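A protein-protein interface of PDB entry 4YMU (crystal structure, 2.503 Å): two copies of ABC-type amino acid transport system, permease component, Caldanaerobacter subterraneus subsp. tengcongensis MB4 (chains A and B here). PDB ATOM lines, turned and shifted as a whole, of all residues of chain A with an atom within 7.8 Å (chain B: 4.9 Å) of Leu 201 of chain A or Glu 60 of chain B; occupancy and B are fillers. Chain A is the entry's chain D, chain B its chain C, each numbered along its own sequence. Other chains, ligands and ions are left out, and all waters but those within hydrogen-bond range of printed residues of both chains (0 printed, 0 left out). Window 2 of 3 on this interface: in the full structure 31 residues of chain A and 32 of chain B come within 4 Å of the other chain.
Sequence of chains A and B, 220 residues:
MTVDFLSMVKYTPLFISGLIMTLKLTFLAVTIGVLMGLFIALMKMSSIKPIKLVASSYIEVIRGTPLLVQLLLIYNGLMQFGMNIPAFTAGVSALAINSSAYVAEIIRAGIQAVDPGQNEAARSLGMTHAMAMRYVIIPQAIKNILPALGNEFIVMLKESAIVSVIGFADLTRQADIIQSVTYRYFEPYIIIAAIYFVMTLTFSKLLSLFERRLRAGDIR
Hydrophobic or aromatic side chains of chain A within 4 Å of the printed part of chain B: Phe 197 and Leu 201. Among the printed residues, 8 pairs touch across the chains.
Printed residues of chain B within 4 Å of Thr 200 of chain A: Gly 64. Leu 201 of chain A touches one residue of chain B. Of chain A, only Phe 197 (3.3 Å) and Leu 201 (3.5 Å) come within 4 Å of Glu 60 of chain B. Printed residues of chain A within 4 Å of Arg 63 of chain B: Lys 158 (2.5 Å). The nearest residue of chain A that does not touch Glu 60 of chain B is Thr 200 of chain A (5.9 Å).
C of Gly 64 of chain B touches CD of Lys 158 of chain A (3.7 Å). O of Tyr 196 of chain A touches O of Gly 64 of chain B (3.7 Å). O of Glu 60 of chain B touches CE1 of Phe 197 of chain A, 3.3 Å away. CE1 of Phe 197 of chain A touches CA of Val 61 of chain B, at 3.5 Å. Gly 64 of chain B touches Phe 197 of chain A. Leu 201 of chain A touches Glu 60 of chain B.
No position is printed for both chains.
The backbone carbonyl oxygen of Arg 63 of chain B lies within hydrogen-bond range of the side-chain amino group of Lys 158 of chain A, 2.5 Å away. OG1 of Thr 200 of chain A is in hydrogen-bond range of O of Gly 64 of chain B (2.8 Å).
O of Tyr 196 of chain A is in hydrogen-bond range of OG1 of Thr 200 of chain A, at 3.3 Å. O of Thr 200 of chain A lies within hydrogen-bond range of OG of Ser 204 of chain A, at 3.1 Å.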
ATOM      1  N   ILE A 154     -22.268 -21.622  -0.571  1.00  0.00           N
ATOM      2  CA  ILE A 154     -20.894 -21.764  -0.098  1.00  0.00           C
ATOM      3  C   ILE A 154     -20.560 -20.662   0.903  1.00  0.00           C
ATOM      4  O   ILE A 154     -19.957 -20.922   1.944  1.00  0.00           O
ATOM      5  CB  ILE A 154     -19.877 -21.745  -1.265  1.00  0.00           C
ATOM      6  CG1 ILE A 154     -20.070 -22.971  -2.167  1.00  0.00           C
ATOM      7  CG2 ILE A 154     -18.444 -21.676  -0.746  1.00  0.00           C
ATOM      8  CD1 ILE A 154     -19.113 -23.026  -3.334  1.00  0.00           C
ATOM      9  N   LEU A 157     -22.207 -21.163   4.380  1.00  0.00           N
ATOM     10  CA  LEU A 157     -21.554 -22.150   5.242  1.00  0.00           C
ATOM     11  C   LEU A 157     -20.658 -21.417   6.217  1.00  0.00           C
ATOM     12  O   LEU A 157     -20.732 -21.621   7.430  1.00  0.00           O
ATOM     13  CB  LEU A 157     -20.714 -23.134   4.427  1.00  0.00           C
ATOM     14  CG  LEU A 157     -21.496 -24.246   3.724  1.00  0.00           C
ATOM     15  CD1 LEU A 157     -20.547 -25.214   3.040  1.00  0.00           C
ATOM     16  CD2 LEU A 157     -22.389 -24.987   4.715  1.00  0.00           C
ATOM     17  N   LYS A 158     -19.803 -20.564   5.681  1.00  0.00           N
ATOM     18  CA  LYS A 158     -18.967 -19.749   6.531  1.00  0.00           C
ATOM     19  C   LYS A 158     -19.853 -18.877   7.422  1.00  0.00           C
ATOM     20  O   LYS A 158     -19.631 -18.778   8.631  1.00  0.00           O
ATOM     21  CB  LYS A 158     -18.017 -18.896   5.687  1.00  0.00           C
ATOM     22  CG  LYS A 158     -17.025 -19.719   4.889  1.00  0.00           C
ATOM     23  CD  LYS A 158     -15.917 -18.856   4.284  1.00  0.00           C
ATOM     24  CE  LYS A 158     -16.461 -17.916   3.208  1.00  0.00           C
ATOM     25  NZ  LYS A 158     -15.458 -16.871   2.818  1.00  0.00           N
ATOM     26  N   ALA A 194      -9.820 -26.085   9.420  1.00  0.00           N
ATOM     27  CA  ALA A 194      -9.519 -27.081   8.397  1.00  0.00           C
ATOM     28  C   ALA A 194     -10.785 -27.726   7.822  1.00  0.00           C
ATOM     29  O   ALA A 194     -10.914 -27.853   6.603  1.00  0.00           O
ATOM     30  CB  ALA A 194      -8.579 -28.142   8.939  1.00  0.00           C
ATOM     31  N   ILE A 195     -11.720 -28.125   8.677  1.00  0.00           N
ATOM     32  CA  ILE A 195     -12.958 -28.708   8.164  1.00  0.00           C
ATOM     33  C   ILE A 195     -13.723 -27.698   7.291  1.00  0.00           C
ATOM     34  O   ILE A 195     -14.250 -28.056   6.229  1.00  0.00           O
ATOM     35  CB  ILE A 195     -13.889 -29.226   9.287  1.00  0.00           C
ATOM     36  CG1 ILE A 195     -13.217 -30.335  10.091  1.00  0.00           C
ATOM     37  CG2 ILE A 195     -15.174 -29.778   8.716  1.00  0.00           C
ATOM     38  CD1 ILE A 195     -14.152 -30.987  11.107  1.00  0.00           C
ATOM     39  N   TYR A 196     -13.779 -26.442   7.734  1.00  0.00           N
ATOM     40  CA  TYR A 196     -14.455 -25.391   6.971  1.00  0.00           C
ATOM     41  C   TYR A 196     -13.792 -25.229   5.611  1.00  0.00           C
ATOM     42  O   TYR A 196     -14.468 -25.095   4.603  1.00  0.00           O
ATOM     43  CB  TYR A 196     -14.441 -24.043   7.715  1.00  0.00           C
ATOM     44  CG  TYR A 196     -15.598 -23.846   8.682  1.00  0.00           C
ATOM     45  CD1 TYR A 196     -16.899 -23.710   8.217  1.00  0.00           C
ATOM     46  CD2 TYR A 196     -15.383 -23.795  10.063  1.00  0.00           C
ATOM     47  CE1 TYR A 196     -17.960 -23.532   9.095  1.00  0.00           C
ATOM     48  CE2 TYR A 196     -16.443 -23.617  10.960  1.00  0.00           C
ATOM     49  CZ  TYR A 196     -17.731 -23.490  10.473  1.00  0.00           C
ATOM     50  OH  TYR A 196     -18.789 -23.315  11.352  1.00  0.00           O
ATOM     51  N   PHE A 197     -12.468 -25.268   5.603  1.00  0.00           N
ATOM     52  CA  PHE A 197     -11.688 -25.098   4.397  1.00  0.00           C
ATOM     53  C   PHE A 197     -11.978 -26.215   3.409  1.00  0.00           C
ATOM     54  O   PHE A 197     -12.274 -25.960   2.237  1.00  0.00           O
ATOM     55  CB  PHE A 197     -10.206 -25.075   4.716  1.00  0.00           C
ATOM     56  CG  PHE A 197      -9.349 -24.801   3.518  1.00  0.00           C
ATOM     57  CD1 PHE A 197      -9.289 -23.528   2.970  1.00  0.00           C
ATOM     58  CD2 PHE A 197      -8.629 -25.822   2.914  1.00  0.00           C
ATOM     59  CE1 PHE A 197      -8.503 -23.270   1.859  1.00  0.00           C
ATOM     60  CE2 PHE A 197      -7.843 -25.569   1.800  1.00  0.00           C
ATOM     61  CZ  PHE A 197      -7.780 -24.292   1.273  1.00  0.00           C
ATOM     62  N   VAL A 198     -11.875 -27.452   3.883  1.00  0.00           N
ATOM     63  CA  VAL A 198     -12.131 -28.605   3.033  1.00  0.00           C
ATOM     64  C   VAL A 198     -13.561 -28.587   2.478  1.00  0.00           C
ATOM     65  O   VAL A 198     -13.788 -28.930   1.313  1.00  0.00           O
ATOM     66  CB  VAL A 198     -11.775 -29.927   3.747  1.00  0.00           C
ATOM     67  CG1 VAL A 198     -12.591 -31.080   3.211  1.00  0.00           C
ATOM     68  CG2 VAL A 198     -10.275 -30.193   3.606  1.00  0.00           C
ATOM     69  N   MET A 199     -14.515 -28.155   3.295  1.00  0.00           N
ATOM     70  CA  MET A 199     -15.891 -28.011   2.823  1.00  0.00           C
ATOM     71  C   MET A 199     -15.984 -26.974   1.699  1.00  0.00           C
ATOM     72  O   MET A 199     -16.647 -27.194   0.670  1.00  0.00           O
ATOM     73  CB  MET A 199     -16.808 -27.598   3.967  1.00  0.00           C
ATOM     74  CG  MET A 199     -17.918 -28.579   4.250  1.00  0.00           C
ATOM     75  SD  MET A 199     -19.025 -27.876   5.477  1.00  0.00           S
ATOM     76  CE  MET A 199     -17.819 -27.133   6.588  1.00  0.00           C
ATOM     77  N   THR A 200     -15.329 -25.837   1.924  1.00  0.00           N
ATOM     78  CA  THR A 200     -15.319 -24.748   0.972  1.00  0.00           C
ATOM     79  C   THR A 200     -14.773 -25.230  -0.373  1.00  0.00           C
ATOM     80  O   THR A 200     -15.418 -25.052  -1.403  1.00  0.00           O
ATOM     81  CB  THR A 200     -14.474 -23.571   1.498  1.00  0.00           C
ATOM     82  OG1 THR A 200     -15.268 -22.773   2.381  1.00  0.00           O
ATOM     83  CG2 THR A 200     -13.956 -22.699   0.338  1.00  0.00           C
ATOM     84  N   LEU A 201     -13.602 -25.868  -0.344  1.00  0.00           N
ATOM     85  CA  LEU A 201     -12.971 -26.432  -1.533  1.00  0.00           C
ATOM     86  C   LEU A 201     -13.882 -27.421  -2.243  1.00  0.00           C
ATOM     87  O   LEU A 201     -14.069 -27.340  -3.460  1.00  0.00           O
ATOM     88  CB  LEU A 201     -11.669 -27.139  -1.179  1.00  0.00           C
ATOM     89  CG  LEU A 201     -10.414 -26.312  -0.916  1.00  0.00           C
ATOM     90  CD1 LEU A 201      -9.233 -27.247  -0.877  1.00  0.00           C
ATOM     91  CD2 LEU A 201     -10.204 -25.229  -1.958  1.00  0.00           C
ATOM     92  N   THR A 202     -14.410 -28.383  -1.491  1.00  0.00           N
ATOM     93  CA  THR A 202     -15.282 -29.398  -2.071  1.00  0.00           C
ATOM     94  C   THR A 202     -16.431 -28.763  -2.854  1.00  0.00           C
ATOM     95  O   THR A 202     -16.586 -28.998  -4.065  1.00  0.00           O
ATOM     96  CB  THR A 202     -15.856 -30.330  -0.986  1.00  0.00           C
ATOM     97  OG1 THR A 202     -14.784 -30.994  -0.309  1.00  0.00           O
ATOM     98  CG2 THR A 202     -16.786 -31.362  -1.596  1.00  0.00           C
ATOM     99  N   PHE A 203     -17.215 -27.935  -2.169  1.00  0.00           N
ATOM    100  CA  PHE A 203     -18.385 -27.330  -2.801  1.00  0.00           C
ATOM    101  C   PHE A 203     -18.031 -26.356  -3.933  1.00  0.00           C
ATOM    102  O   PHE A 203     -18.806 -26.190  -4.873  1.00  0.00           O
ATOM    103  CB  PHE A 203     -19.281 -26.648  -1.773  1.00  0.00           C
ATOM    104  CG  PHE A 203     -20.057 -27.606  -0.908  1.00  0.00           C
ATOM    105  CD1 PHE A 203     -20.895 -28.557  -1.475  1.00  0.00           C
ATOM    106  CD2 PHE A 203     -19.993 -27.522   0.483  1.00  0.00           C
ATOM    107  CE1 PHE A 203     -21.637 -29.434  -0.669  1.00  0.00           C
ATOM    108  CE2 PHE A 203     -20.735 -28.389   1.297  1.00  0.00           C
ATOM    109  CZ  PHE A 203     -21.559 -29.345   0.720  1.00  0.00           C
ATOM    110  N   SER A 204     -16.869 -25.714  -3.838  1.00  0.00           N
ATOM    111  CA  SER A 204     -16.407 -24.804  -4.879  1.00  0.00           C
ATOM    112  C   SER A 204     -16.095 -25.566  -6.159  1.00  0.00           C
ATOM    113  O   SER A 204     -16.479 -25.153  -7.267  1.00  0.00           O
ATOM    114  CB  SER A 204     -15.156 -24.070  -4.413  1.00  0.00           C
ATOM    115  OG  SER A 204     -15.490 -22.908  -3.679  1.00  0.00           O
ATOM    116  N   LYS A 205     -15.367 -26.664  -5.990  1.00  0.00           N
ATOM    117  CA  LYS A 205     -15.067 -27.581  -7.076  1.00  0.00           C
ATOM    118  C   LYS A 205     -16.353 -28.051  -7.754  1.00  0.00           C
ATOM    119  O   LYS A 205     -16.527 -27.879  -8.975  1.00  0.00           O
ATOM    120  CB  LYS A 205     -14.242 -28.763  -6.555  1.00  0.00           C
ATOM    121  CG  LYS A 205     -14.136 -29.952  -7.500  1.00  0.00           C
ATOM    122  CD  LYS A 205     -14.494 -31.262  -6.793  1.00  0.00           C
ATOM    123  CE  LYS A 205     -13.354 -31.720  -5.869  1.00  0.00           C
ATOM    124  NZ  LYS A 205     -13.522 -33.116  -5.356  1.00  0.00           N
ATOM    125  N   LEU A 206     -17.280 -28.555  -6.981  1.00  0.00           N
ATOM    126  CA  LEU A 206     -18.513 -28.984  -7.573  1.00  0.00           C
ATOM    127  C   LEU A 206     -19.178 -27.876  -8.345  1.00  0.00           C
ATOM    128  O   LEU A 206     -19.590 -28.084  -9.465  1.00  0.00           O
ATOM    129  CB  LEU A 206     -19.449 -29.511  -6.511  1.00  0.00           C
ATOM    130  CG  LEU A 206     -19.190 -30.982  -6.237  1.00  0.00           C
ATOM    131  CD1 LEU A 206     -18.724 -31.198  -4.810  1.00  0.00           C
ATOM    132  CD2 LEU A 206     -20.450 -31.768  -6.524  1.00  0.00           C
ATOM    133  N   LEU A 207     -19.295 -26.703  -7.751  1.00  0.00           N
ATOM    134  CA  LEU A 207     -20.100 -25.676  -8.360  1.00  0.00           C
ATOM    135  C   LEU A 207     -19.557 -25.263  -9.708  1.00  0.00           C
ATOM    136  O   LEU A 207     -20.300 -25.210 -10.673  1.00  0.00           O
ATOM    137  CB  LEU A 207     -20.166 -24.475  -7.439  1.00  0.00           C
ATOM    138  CG  LEU A 207     -20.174 -23.066  -7.999  1.00  0.00           C
ATOM    139  CD1 LEU A 207     -21.572 -22.569  -8.261  1.00  0.00           C
ATOM    140  CD2 LEU A 207     -19.461 -22.129  -7.063  1.00  0.00           C
ATOM    141  N   SER B  56      -0.425 -17.883  -2.036  1.00  0.00           N
ATOM    142  CA  SER B  56      -1.625 -18.521  -2.565  1.00  0.00           C
ATOM    143  C   SER B  56      -2.356 -19.308  -1.474  1.00  0.00           C
ATOM    144  O   SER B  56      -3.587 -19.250  -1.361  1.00  0.00           O
ATOM    145  CB  SER B  56      -1.248 -19.462  -3.702  1.00  0.00           C
ATOM    146  OG  SER B  56      -0.840 -18.725  -4.836  1.00  0.00           O
ATOM    147  N   SER B  57      -1.585 -20.038  -0.672  1.00  0.00           N
ATOM    148  CA  SER B  57      -2.141 -20.856   0.400  1.00  0.00           C
ATOM    149  C   SER B  57      -2.777 -19.986   1.470  1.00  0.00           C
ATOM    150  O   SER B  57      -3.890 -20.251   1.909  1.00  0.00           O
ATOM    151  CB  SER B  57      -1.055 -21.728   1.026  1.00  0.00           C
ATOM    152  OG  SER B  57      -0.702 -22.793   0.166  1.00  0.00           O
ATOM    153  N   TYR B  58      -2.052 -18.950   1.869  1.00  0.00           N
ATOM    154  CA  TYR B  58      -2.529 -17.944   2.803  1.00  0.00           C
ATOM    155  C   TYR B  58      -3.882 -17.402   2.357  1.00  0.00           C
ATOM    156  O   TYR B  58      -4.892 -17.540   3.079  1.00  0.00           O
ATOM    157  CB  TYR B  58      -1.495 -16.826   2.862  1.00  0.00           C
ATOM    158  CG  TYR B  58      -1.811 -15.658   3.761  1.00  0.00           C
ATOM    159  CD1 TYR B  58      -1.313 -15.602   5.055  1.00  0.00           C
ATOM    160  CD2 TYR B  58      -2.560 -14.585   3.302  1.00  0.00           C
ATOM    161  CE1 TYR B  58      -1.577 -14.522   5.874  1.00  0.00           C
ATOM    162  CE2 TYR B  58      -2.828 -13.500   4.116  1.00  0.00           C
ATOM    163  CZ  TYR B  58      -2.333 -13.475   5.399  1.00  0.00           C
ATOM    164  OH  TYR B  58      -2.596 -12.398   6.209  1.00  0.00           O
ATOM    165  N   ILE B  59      -3.909 -16.814   1.158  1.00  0.00           N
ATOM    166  CA  ILE B  59      -5.145 -16.257   0.601  1.00  0.00           C
ATOM    167  C   ILE B  59      -6.297 -17.268   0.603  1.00  0.00           C
ATOM    168  O   ILE B  59      -7.398 -16.979   1.086  1.00  0.00           O
ATOM    169  CB  ILE B  59      -4.936 -15.744  -0.836  1.00  0.00           C
ATOM    170  CG1 ILE B  59      -3.987 -14.545  -0.843  1.00  0.00           C
ATOM    171  CG2 ILE B  59      -6.268 -15.368  -1.475  1.00  0.00           C
ATOM    172  CD1 ILE B  59      -3.570 -14.120  -2.224  1.00  0.00           C
ATOM    173  N   GLU B  60      -6.035 -18.451   0.062  1.00  0.00           N
ATOM    174  CA  GLU B  60      -7.062 -19.476  -0.054  1.00  0.00           C
ATOM    175  C   GLU B  60      -7.634 -19.892   1.307  1.00  0.00           C
ATOM    176  O   GLU B  60      -8.858 -20.029   1.473  1.00  0.00           O
ATOM    177  CB  GLU B  60      -6.514 -20.687  -0.804  1.00  0.00           C
ATOM    178  CG  GLU B  60      -7.597 -21.565  -1.410  1.00  0.00           C
ATOM    179  CD  GLU B  60      -7.058 -22.481  -2.494  1.00  0.00           C
ATOM    180  OE1 GLU B  60      -5.828 -22.702  -2.526  1.00  0.00           O
ATOM    181  OE2 GLU B  60      -7.861 -22.968  -3.323  1.00  0.00           O
ATOM    182  N   VAL B  61      -6.744 -20.105   2.275  1.00  0.00           N
ATOM    183  CA  VAL B  61      -7.155 -20.557   3.599  1.00  0.00           C
ATOM    184  C   VAL B  61      -8.000 -19.496   4.266  1.00  0.00           C
ATOM    185  O   VAL B  61      -9.098 -19.771   4.720  1.00  0.00           O
ATOM    186  CB  VAL B  61      -5.946 -20.882   4.499  1.00  0.00           C
ATOM    187  CG1 VAL B  61      -6.363 -20.914   5.941  1.00  0.00           C
ATOM    188  CG2 VAL B  61      -5.339 -22.212   4.101  1.00  0.00           C
ATOM    189  N   ILE B  62      -7.508 -18.267   4.273  1.00  0.00           N
ATOM    190  CA  ILE B  62      -8.244 -17.203   4.937  1.00  0.00           C
ATOM    191  C   ILE B  62      -9.603 -16.903   4.299  1.00  0.00           C
ATOM    192  O   ILE B  62     -10.584 -16.688   5.005  1.00  0.00           O
ATOM    193  CB  ILE B  62      -7.383 -15.950   5.041  1.00  0.00           C
ATOM    194  CG1 ILE B  62      -6.191 -16.263   5.933  1.00  0.00           C
ATOM    195  CG2 ILE B  62      -8.183 -14.779   5.591  1.00  0.00           C
ATOM    196  CD1 ILE B  62      -5.181 -15.185   5.962  1.00  0.00           C
ATOM    197  N   ARG B  63      -9.683 -16.907   2.971  1.00  0.00           N
ATOM    198  CA  ARG B  63     -10.955 -16.591   2.331  1.00  0.00           C
ATOM    199  C   ARG B  63     -11.933 -17.765   2.384  1.00  0.00           C
ATOM    200  O   ARG B  63     -13.153 -17.576   2.349  1.00  0.00           O
ATOM    201  CB  ARG B  63     -10.731 -16.112   0.889  1.00  0.00           C
ATOM    202  CG  ARG B  63      -9.841 -14.868   0.806  1.00  0.00           C
ATOM    203  CD  ARG B  63      -9.683 -14.363  -0.627  1.00  0.00           C
ATOM    204  NE  ARG B  63     -10.930 -13.850  -1.199  1.00  0.00           N
ATOM    205  CZ  ARG B  63     -11.456 -14.260  -2.347  1.00  0.00           C
ATOM    206  NH1 ARG B  63     -10.858 -15.214  -3.044  1.00  0.00           N
ATOM    207  NH2 ARG B  63     -12.594 -13.736  -2.782  1.00  0.00           N
ATOM    208  N   GLY B  64     -11.408 -18.980   2.478  1.00  0.00           N
ATOM    209  CA  GLY B  64     -12.272 -20.148   2.448  1.00  0.00           C
ATOM    210  C   GLY B  64     -12.700 -20.584   3.841  1.00  0.00           C
ATOM    211  O   GLY B  64     -13.255 -21.676   4.025  1.00  0.00           O
